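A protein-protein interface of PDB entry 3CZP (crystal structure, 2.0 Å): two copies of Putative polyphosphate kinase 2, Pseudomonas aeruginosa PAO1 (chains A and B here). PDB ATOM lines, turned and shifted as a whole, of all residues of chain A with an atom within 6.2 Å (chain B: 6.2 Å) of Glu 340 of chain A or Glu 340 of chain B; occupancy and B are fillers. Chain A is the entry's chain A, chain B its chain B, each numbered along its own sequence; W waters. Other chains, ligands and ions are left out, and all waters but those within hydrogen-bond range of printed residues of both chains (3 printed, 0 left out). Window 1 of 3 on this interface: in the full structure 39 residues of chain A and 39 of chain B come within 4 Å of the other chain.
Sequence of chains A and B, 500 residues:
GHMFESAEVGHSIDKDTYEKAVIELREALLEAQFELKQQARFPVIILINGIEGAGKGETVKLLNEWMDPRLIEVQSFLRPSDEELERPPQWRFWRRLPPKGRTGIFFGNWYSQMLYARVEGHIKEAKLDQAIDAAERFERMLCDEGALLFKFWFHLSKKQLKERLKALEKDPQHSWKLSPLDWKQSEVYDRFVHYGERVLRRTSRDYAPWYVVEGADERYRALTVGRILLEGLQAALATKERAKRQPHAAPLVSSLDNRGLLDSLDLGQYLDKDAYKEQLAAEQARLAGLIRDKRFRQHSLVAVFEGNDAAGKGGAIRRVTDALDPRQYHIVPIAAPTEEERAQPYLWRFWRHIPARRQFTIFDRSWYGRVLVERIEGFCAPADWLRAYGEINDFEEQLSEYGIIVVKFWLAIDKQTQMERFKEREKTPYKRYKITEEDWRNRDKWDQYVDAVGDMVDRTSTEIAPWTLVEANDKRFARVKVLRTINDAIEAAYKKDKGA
Glu 339 of chain B touches Thr 338 of chain A.
Glu 339 of chain A touches Thr 338 of chain B (OE1 to CA, 3.4 Å).
Glu 341 of chain B touches Glu 340 of chain A.
Water W2 lies within hydrogen-bond range of NH1 of Arg 342 of chain B and OE1 of Glu 339 of chain A.
Water W3 lies within hydrogen-bond range of OE1 of Glu 339 of chain A (2.6 Å) and NH2 of Arg 342 of chain B (3.4 Å).
Water W1 lies within hydrogen-bond range of OE2 of Glu 340 of chain A (2.8 Å) and NH2 of Arg 352 of chain B (3.0 Å).
Printed residues of chain B within 4 Å of Glu 340 of chain A: Thr 338 (2.6 Å), Glu 340 (3.2 Å), Glu 341 (3.95 Å) and Arg 352 (3.1 Å).
Printed residues of chain A within 4 Å of Glu 340 of chain B: Thr 338, Glu 340 and Arg 352.
Of the printed residues of chain A, Arg 352 of chain B touches Glu 340.
Printed residues of chain B within 4 Å of Thr 338 of chain A: Glu 339 and Glu 340.
Printed residues of chain B within 4 Å of Arg 352 of chain A: Glu 340 (2.8 Å).
Of the printed residues of chain A, Arg 342 of chain B touches Glu 339 (3.7 Å).
Of the printed residues of chain A, Glu 341 of chain B touches Glu 340 (3.95 Å).
Ala 343 of chain B touches none of the printed residues of chain A.
The nearest printed residue of chain A that does not touch Glu 340 of chain B is Glu 341 of chain A (4.03 Å).
The nearest printed residue of chain B that does not touch Glu 339 of chain A is Glu 340 of chain B (5.4 Å).
Of the 10 printed residues of chain A, 5 touch a printed residue of chain B.
Along chain A the printed residues that touch a printed residue of chain B span positions 338 to 352.
Printed residues of chain B that touch a printed residue of chain A: Thr 338, Glu 339, Glu 340, Glu 341, Arg 342 and Arg 352.
Among the printed residues, 11 pairs touch across the chains.
Among the printed residues, Asp or Glu carboxylates within 4 Å of a Lys or Arg side-chain nitrogen of the other chain: Glu 339 of chain A with Arg 342 of chain B, Glu 340 of chain A with Arg 352 of chain B, Arg 342 of chain A with Glu 339 of chain B and Arg 352 of chain A with Glu 340 of chain B.
The guanidinium group of Arg 342 of chain B lies within salt-bridge range of the side-chain carboxylate of Glu 339 of chain A (3.7 Å).
The guanidinium group (NH2) of Arg 352 of chain A lies within salt-bridge range of the side-chain carboxylate (OE2) of Glu 340 of chain B (2.8 Å).
The side-chain carboxylate of Glu 340 of chain B lies within hydrogen-bond range of the side-chain hydroxyl of Thr 338 of chain A.
The backbone NH of Glu 339 of chain A sits at hydrogen-bond distance from the side-chain carboxylate of Glu 339 of chain B (2.9 Å).
OE1 of Glu 340 of chain A is in salt-bridge range of NH1 of Arg 352 of chain B (3.1 Å).
The side-chain carboxylate (OE1) of Glu 340 of chain A lies within hydrogen-bond range of the side-chain hydroxyl (OG1) of Thr 338 of chain B (2.6 Å).
The side-chain carboxylate (OE2) of Glu 340 of chain A sits close to the side-chain carboxylate (OE2) of Glu 340 of chain B.
The guanidinium group of Arg 342 of chain A is in salt-bridge range of the side-chain carboxylate of Glu 339 of chain B, 3.7 Å away.
OE2 of Glu 341 of chain A is in salt-bridge range of NH1 of Arg 352 of chain A (2.9 Å).
The backbone NH (N) of Thr 338 of chain B is in hydrogen-bond range of the side-chain carboxylate (OE1) of Glu 341 of chain B (2.8 Å).
OE1 of Glu 341 of chain A lies within hydrogen-bond range of N of Thr 338 of chain A (2.8 Å).
The guanidinium group (NH1) of Arg 352 of chain B lies within salt-bridge range of the side-chain carboxylate (OE2) of Glu 341 of chain B, 3.2 Å away.
Thr 338 of chain A touches Glu 339 of chain B, and with the chains exchanged Glu 339 of chain A touches Thr 338 of chain B.
Thr 338 of chain A touches Glu 340 of chain B, and with the chains exchanged Glu 340 of chain A touches Thr 338 of chain B.
Glu 339 of chain A touches its own counterpart, Glu 339 of chain B.
Glu 340 of chain A touches Glu 341 of chain B, but with the chains exchanged Glu 341 of chain A does not touch Glu 340 of chain B (4.03 Å).
Of the 11 pairs that touch across the chains among the printed residues, 10 have their exchanged pair printed and touching as well.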
ATOM      1  N   PRO A  99      -0.623 -11.024 -21.345  1.00  0.00           N
ATOM      2  CA  PRO A  99      -0.681 -10.722 -22.761  1.00  0.00           C
ATOM      3  C   PRO A  99       0.672 -10.915 -23.477  1.00  0.00           C
ATOM      4  O   PRO A  99       1.753 -10.932 -22.858  1.00  0.00           O
ATOM      5  CB  PRO A  99      -1.116  -9.251 -22.786  1.00  0.00           C
ATOM      6  CG  PRO A  99      -0.873  -8.727 -21.375  1.00  0.00           C
ATOM      7  CD  PRO A  99      -0.773  -9.862 -20.458  1.00  0.00           C
ATOM      8  N   THR A 338     -11.039  -7.586 -30.446  1.00  0.00           N
ATOM      9  CA  THR A 338     -10.468  -6.304 -30.049  1.00  0.00           C
ATOM     10  C   THR A 338      -8.959  -6.495 -29.759  1.00  0.00           C
ATOM     11  O   THR A 338      -8.447  -7.623 -29.776  1.00  0.00           O
ATOM     12  CB  THR A 338     -11.200  -5.749 -28.800  1.00  0.00           C
ATOM     13  OG1 THR A 338     -10.996  -6.664 -27.716  1.00  0.00           O
ATOM     14  CG2 THR A 338     -12.652  -5.653 -29.016  1.00  0.00           C
ATOM     15  N   GLU A 339      -8.264  -5.404 -29.530  1.00  0.00           N
ATOM     16  CA  GLU A 339      -6.812  -5.399 -29.257  1.00  0.00           C
ATOM     17  C   GLU A 339      -6.394  -6.296 -28.066  1.00  0.00           C
ATOM     18  O   GLU A 339      -5.417  -7.074 -28.137  1.00  0.00           O
ATOM     19  CB  GLU A 339      -6.390  -3.928 -29.047  1.00  0.00           C
ATOM     20  CG  GLU A 339      -5.122  -3.673 -28.295  1.00  0.00           C
ATOM     21  CD  GLU A 339      -4.519  -2.303 -28.616  1.00  0.00           C
ATOM     22  OE1 GLU A 339      -5.296  -1.369 -28.949  1.00  0.00           O
ATOM     23  OE2 GLU A 339      -3.271  -2.219 -28.564  1.00  0.00           O
ATOM     24  N   GLU A 340      -7.154  -6.179 -26.978  1.00  0.00           N
ATOM     25  CA  GLU A 340      -6.923  -6.958 -25.766  1.00  0.00           C
ATOM     26  C   GLU A 340      -7.255  -8.436 -25.938  1.00  0.00           C
ATOM     27  O   GLU A 340      -6.703  -9.259 -25.199  1.00  0.00           O
ATOM     28  CB  GLU A 340      -7.678  -6.349 -24.563  1.00  0.00           C
ATOM     29  CG  GLU A 340      -6.903  -5.206 -23.901  1.00  0.00           C
ATOM     30  CD  GLU A 340      -7.664  -4.421 -22.821  1.00  0.00           C
ATOM     31  OE1 GLU A 340      -7.242  -3.282 -22.593  1.00  0.00           O
ATOM     32  OE2 GLU A 340      -8.640  -4.922 -22.196  1.00  0.00           O
ATOM     33  N   GLU A 341      -8.163  -8.771 -26.873  1.00  0.00           N
ATOM     34  CA  GLU A 341      -8.424 -10.137 -27.265  1.00  0.00           C
ATOM     35  C   GLU A 341      -7.357 -10.719 -28.199  1.00  0.00           C
ATOM     36  O   GLU A 341      -7.034 -11.910 -28.119  1.00  0.00           O
ATOM     37  CB  GLU A 341      -9.751 -10.259 -27.971  1.00  0.00           C
ATOM     38  CG  GLU A 341     -10.911 -10.007 -26.975  1.00  0.00           C
ATOM     39  CD  GLU A 341     -12.222  -9.799 -27.645  1.00  0.00           C
ATOM     40  OE1 GLU A 341     -12.277  -9.505 -28.892  1.00  0.00           O
ATOM     41  OE2 GLU A 341     -13.209  -9.868 -26.895  1.00  0.00           O
ATOM     42  N   ARG A 342      -6.834  -9.880 -29.079  1.00  0.00           N
ATOM     43  CA  ARG A 342      -5.796 -10.317 -29.986  1.00  0.00           C
ATOM     44  C   ARG A 342      -4.434 -10.623 -29.262  1.00  0.00           C
ATOM     45  O   ARG A 342      -3.629 -11.420 -29.745  1.00  0.00           O
ATOM     46  CB  ARG A 342      -5.627  -9.274 -31.067  1.00  0.00           C
ATOM     47  CG  ARG A 342      -6.750  -9.279 -32.127  1.00  0.00           C
ATOM     48  CD  ARG A 342      -6.362  -8.438 -33.381  1.00  0.00           C
ATOM     49  NE  ARG A 342      -5.812  -7.110 -33.010  1.00  0.00           N
ATOM     50  CZ  ARG A 342      -6.495  -5.951 -32.929  1.00  0.00           C
ATOM     51  NH1 ARG A 342      -7.796  -5.848 -33.231  1.00  0.00           N
ATOM     52  NH2 ARG A 342      -5.855  -4.839 -32.565  1.00  0.00           N
ATOM     53  N   ALA A 343      -4.203  -9.991 -28.108  1.00  0.00           N
ATOM     54  CA  ALA A 343      -2.990 -10.176 -27.286  1.00  0.00           C
ATOM     55  C   ALA A 343      -3.062 -11.472 -26.495  1.00  0.00           C
ATOM     56  O   ALA A 343      -2.142 -11.786 -25.743  1.00  0.00           O
ATOM     57  CB  ALA A 343      -2.831  -9.011 -26.340  1.00  0.00           C
ATOM     58  N   GLN A 344      -4.142 -12.252 -26.668  1.00  0.00           N
ATOM     59  CA  GLN A 344      -4.380 -13.465 -25.826  1.00  0.00           C
ATOM     60  C   GLN A 344      -4.691 -14.667 -26.736  1.00  0.00           C
ATOM     61  O   GLN A 344      -4.962 -14.503 -27.921  1.00  0.00           O
ATOM     62  CB  GLN A 344      -5.538 -13.184 -24.926  1.00  0.00           C
ATOM     63  CG  GLN A 344      -5.292 -12.103 -23.962  1.00  0.00           C
ATOM     64  CD  GLN A 344      -4.472 -12.585 -22.752  1.00  0.00           C
ATOM     65  OE1 GLN A 344      -4.252 -13.781 -22.598  1.00  0.00           O
ATOM     66  NE2 GLN A 344      -4.004 -11.676 -21.954  1.00  0.00           N
ATOM     67  N   TRP A 348      -9.635 -17.261 -24.940  1.00  0.00           N
ATOM     68  CA  TRP A 348      -9.691 -16.226 -23.906  1.00  0.00           C
ATOM     69  C   TRP A 348     -10.888 -15.278 -24.052  1.00  0.00           C
ATOM     70  O   TRP A 348     -11.566 -14.945 -23.058  1.00  0.00           O
ATOM     71  CB  TRP A 348      -8.347 -15.456 -23.902  1.00  0.00           C
ATOM     72  CG  TRP A 348      -8.181 -14.457 -22.804  1.00  0.00           C
ATOM     73  CD1 TRP A 348      -7.574 -14.628 -21.587  1.00  0.00           C
ATOM     74  CD2 TRP A 348      -8.536 -13.077 -22.875  1.00  0.00           C
ATOM     75  NE1 TRP A 348      -7.599 -13.468 -20.862  1.00  0.00           N
ATOM     76  CE2 TRP A 348      -8.161 -12.485 -21.641  1.00  0.00           C
ATOM     77  CE3 TRP A 348      -9.133 -12.279 -23.855  1.00  0.00           C
ATOM     78  CZ2 TRP A 348      -8.378 -11.130 -21.367  1.00  0.00           C
ATOM     79  CZ3 TRP A 348      -9.308 -10.913 -23.590  1.00  0.00           C
ATOM     80  CH2 TRP A 348      -8.944 -10.366 -22.351  1.00  0.00           C
ATOM     81  N   ARG A 352     -14.112 -15.240 -21.113  1.00  0.00           N
ATOM     82  CA  ARG A 352     -14.343 -13.994 -20.396  1.00  0.00           C
ATOM     83  C   ARG A 352     -15.822 -13.717 -20.343  1.00  0.00           C
ATOM     84  O   ARG A 352     -16.273 -12.973 -19.510  1.00  0.00           O
ATOM     85  CB  ARG A 352     -13.572 -12.808 -21.038  1.00  0.00           C
ATOM     86  CG  ARG A 352     -14.241 -12.291 -22.268  1.00  0.00           C
ATOM     87  CD  ARG A 352     -13.459 -11.258 -23.066  1.00  0.00           C
ATOM     88  NE  ARG A 352     -13.213  -9.990 -22.363  1.00  0.00           N
ATOM     89  CZ  ARG A 352     -12.730  -8.899 -22.972  1.00  0.00           C
ATOM     90  NH1 ARG A 352     -12.462  -8.910 -24.275  1.00  0.00           N
ATOM     91  NH2 ARG A 352     -12.473  -7.794 -22.292  1.00  0.00           N
ATOM     92  N   PRO B  99     -19.563   0.254 -23.418  1.00  0.00           N
ATOM     93  CA  PRO B  99     -18.633   0.907 -24.317  1.00  0.00           C
ATOM     94  C   PRO B  99     -19.329   1.848 -25.284  1.00  0.00           C
ATOM     95  O   PRO B  99     -20.558   1.806 -25.494  1.00  0.00           O
ATOM     96  CB  PRO B  99     -17.949  -0.254 -25.033  1.00  0.00           C
ATOM     97  CG  PRO B  99     -18.900  -1.372 -24.951  1.00  0.00           C
ATOM     98  CD  PRO B  99     -19.705  -1.182 -23.670  1.00  0.00           C
ATOM     99  N   THR B 338      -5.314   1.109 -24.910  1.00  0.00           N
ATOM    100  CA  THR B 338      -5.743   0.072 -25.847  1.00  0.00           C
ATOM    101  C   THR B 338      -7.180   0.328 -26.350  1.00  0.00           C
ATOM    102  O   THR B 338      -7.894   1.172 -25.828  1.00  0.00           O
ATOM    103  CB  THR B 338      -5.690  -1.303 -25.182  1.00  0.00           C
ATOM    104  OG1 THR B 338      -6.516  -1.273 -24.011  1.00  0.00           O
ATOM    105  CG2 THR B 338      -4.300  -1.661 -24.808  1.00  0.00           C
ATOM    106  N   GLU B 339      -7.558  -0.393 -27.392  1.00  0.00           N
ATOM    107  CA  GLU B 339      -8.862  -0.299 -28.002  1.00  0.00           C
ATOM    108  C   GLU B 339      -9.988  -0.273 -26.958  1.00  0.00           C
ATOM    109  O   GLU B 339     -10.790   0.654 -26.943  1.00  0.00           O
ATOM    110  CB  GLU B 339      -9.005  -1.451 -28.969  1.00  0.00           C
ATOM    111  CG  GLU B 339      -9.877  -1.172 -30.089  1.00  0.00           C
ATOM    112  CD  GLU B 339     -10.250  -2.430 -30.850  1.00  0.00           C
ATOM    113  OE1 GLU B 339      -9.351  -3.253 -31.096  1.00  0.00           O
ATOM    114  OE2 GLU B 339     -11.440  -2.558 -31.220  1.00  0.00           O
ATOM    115  N   GLU B 340     -10.022  -1.259 -26.064  1.00  0.00           N
ATOM    116  CA  GLU B 340     -11.071  -1.355 -25.068  1.00  0.00           C
ATOM    117  C   GLU B 340     -11.066  -0.208 -24.097  1.00  0.00           C
ATOM    118  O   GLU B 340     -12.118   0.248 -23.687  1.00  0.00           O
ATOM    119  CB  GLU B 340     -11.078  -2.727 -24.352  1.00  0.00           C
ATOM    120  CG  GLU B 340     -11.518  -3.914 -25.319  1.00  0.00           C
ATOM    121  CD  GLU B 340     -11.543  -5.299 -24.634  1.00  0.00           C
ATOM    122  OE1 GLU B 340     -11.503  -6.384 -25.307  1.00  0.00           O
ATOM    123  OE2 GLU B 340     -11.607  -5.314 -23.387  1.00  0.00           O
ATOM    124  N   GLU B 341      -9.887   0.308 -23.760  1.00  0.00           N
ATOM    125  CA  GLU B 341      -9.770   1.499 -22.928  1.00  0.00           C
ATOM    126  C   GLU B 341     -10.266   2.763 -23.598  1.00  0.00           C
ATOM    127  O   GLU B 341     -10.783   3.674 -22.936  1.00  0.00           O
ATOM    128  CB  GLU B 341      -8.313   1.677 -22.466  1.00  0.00           C
ATOM    129  CG  GLU B 341      -7.810   0.508 -21.621  1.00  0.00           C
ATOM    130  CD  GLU B 341      -6.304   0.568 -21.316  1.00  0.00           C
ATOM    131  OE1 GLU B 341      -5.501   1.139 -22.079  1.00  0.00           O
ATOM    132  OE2 GLU B 341      -5.960   0.026 -20.279  1.00  0.00           O
ATOM    133  N   ARG B 342     -10.036   2.873 -24.897  1.00  0.00           N
ATOM    134  CA  ARG B 342     -10.458   4.054 -25.658  1.00  0.00           C
ATOM    135  C   ARG B 342     -11.943   4.093 -25.843  1.00  0.00           C
ATOM    136  O   ARG B 342     -12.447   5.149 -26.206  1.00  0.00           O
ATOM    137  CB  ARG B 342      -9.826   4.110 -27.072  1.00  0.00           C
ATOM    138  CG  ARG B 342      -8.303   4.268 -27.008  1.00  0.00           C
ATOM    139  CD  ARG B 342      -7.697   4.563 -28.385  1.00  0.00           C
ATOM    140  NE  ARG B 342      -7.998   3.532 -29.375  1.00  0.00           N
ATOM    141  CZ  ARG B 342      -7.250   2.449 -29.645  1.00  0.00           C
ATOM    142  NH1 ARG B 342      -6.133   2.185 -28.989  1.00  0.00           N
ATOM    143  NH2 ARG B 342      -7.627   1.602 -30.604  1.00  0.00           N
ATOM    144  N   ALA B 343     -12.633   2.951 -25.666  1.00  0.00           N
ATOM    145  CA  ALA B 343     -14.059   2.839 -25.793  1.00  0.00           C
ATOM    146  C   ALA B 343     -14.790   3.258 -24.518  1.00  0.00           C
ATOM    147  O   ALA B 343     -15.978   3.178 -24.446  1.00  0.00           O
ATOM    148  CB  ALA B 343     -14.465   1.403 -26.157  1.00  0.00           C
ATOM    149  N   GLN B 344     -14.043   3.704 -23.536  1.00  0.00           N
ATOM    150  CA  GLN B 344     -14.557   4.035 -22.215  1.00  0.00           C
ATOM    151  C   GLN B 344     -14.071   5.415 -21.802  1.00  0.00           C
ATOM    152  O   GLN B 344     -13.111   5.944 -22.382  1.00  0.00           O
ATOM    153  CB  GLN B 344     -14.024   2.982 -21.243  1.00  0.00           C
ATOM    154  CG  GLN B 344     -14.525   1.586 -21.519  1.00  0.00           C
ATOM    155  CD  GLN B 344     -15.971   1.446 -21.128  1.00  0.00           C
ATOM    156  OE1 GLN B 344     -16.550   2.334 -20.446  1.00  0.00           O
ATOM    157  NE2 GLN B 344     -16.582   0.315 -21.523  1.00  0.00           N
ATOM    158  N   TRP B 348     -11.699   5.108 -16.554  1.00  0.00           N
ATOM    159  CA  TRP B 348     -12.003   3.671 -16.579  1.00  0.00           C
ATOM    160  C   TRP B 348     -10.716   2.837 -16.546  1.00  0.00           C
ATOM    161  O   TRP B 348     -10.612   1.840 -15.806  1.00  0.00           O
ATOM    162  CB  TRP B 348     -12.779   3.357 -17.860  1.00  0.00           C
ATOM    163  CG  TRP B 348     -13.287   1.974 -18.001  1.00  0.00           C
ATOM    164  CD1 TRP B 348     -14.477   1.486 -17.537  1.00  0.00           C
ATOM    165  CD2 TRP B 348     -12.660   0.887 -18.726  1.00  0.00           C
ATOM    166  NE1 TRP B 348     -14.616   0.167 -17.891  1.00  0.00           N
ATOM    167  CE2 TRP B 348     -13.514  -0.219 -18.630  1.00  0.00           C
ATOM    168  CE3 TRP B 348     -11.447   0.749 -19.433  1.00  0.00           C
ATOM    169  CZ2 TRP B 348     -13.207  -1.461 -19.221  1.00  0.00           C
ATOM    170  CZ3 TRP B 348     -11.146  -0.457 -20.022  1.00  0.00           C
ATOM    171  CH2 TRP B 348     -12.017  -1.569 -19.895  1.00  0.00           C
ATOM    172  N   ARG B 352      -9.839   0.203 -13.244  1.00  0.00           N
ATOM    173  CA  ARG B 352      -9.709  -1.247 -13.458  1.00  0.00           C
ATOM    174  C   ARG B 352      -8.494  -1.851 -12.739  1.00  0.00           C
ATOM    175  O   ARG B 352      -8.468  -3.084 -12.509  1.00  0.00           O
ATOM    176  CB  ARG B 352      -9.744  -1.616 -14.971  1.00  0.00           C
ATOM    177  CG  ARG B 352      -8.495  -1.170 -15.667  1.00  0.00           C
ATOM    178  CD  ARG B 352      -8.405  -1.391 -17.179  1.00  0.00           C
ATOM    179  NE  ARG B 352      -8.751  -2.740 -17.609  1.00  0.00           N
ATOM    180  CZ  ARG B 352      -8.460  -3.211 -18.817  1.00  0.00           C
ATOM    181  NH1 ARG B 352      -7.794  -2.479 -19.695  1.00  0.00           N
ATOM    182  NH2 ARG B 352      -8.840  -4.432 -19.154  1.00  0.00           N
HETATM  183  O   HOH W   1      -8.976  -7.121 -20.452  1.00  0.00           O
HETATM  184  O   HOH W   2      -4.268   0.801 -29.993  1.00  0.00           O
HETATM  185  O   HOH W   3      -5.468  -0.853 -31.503  1.00  0.00           O
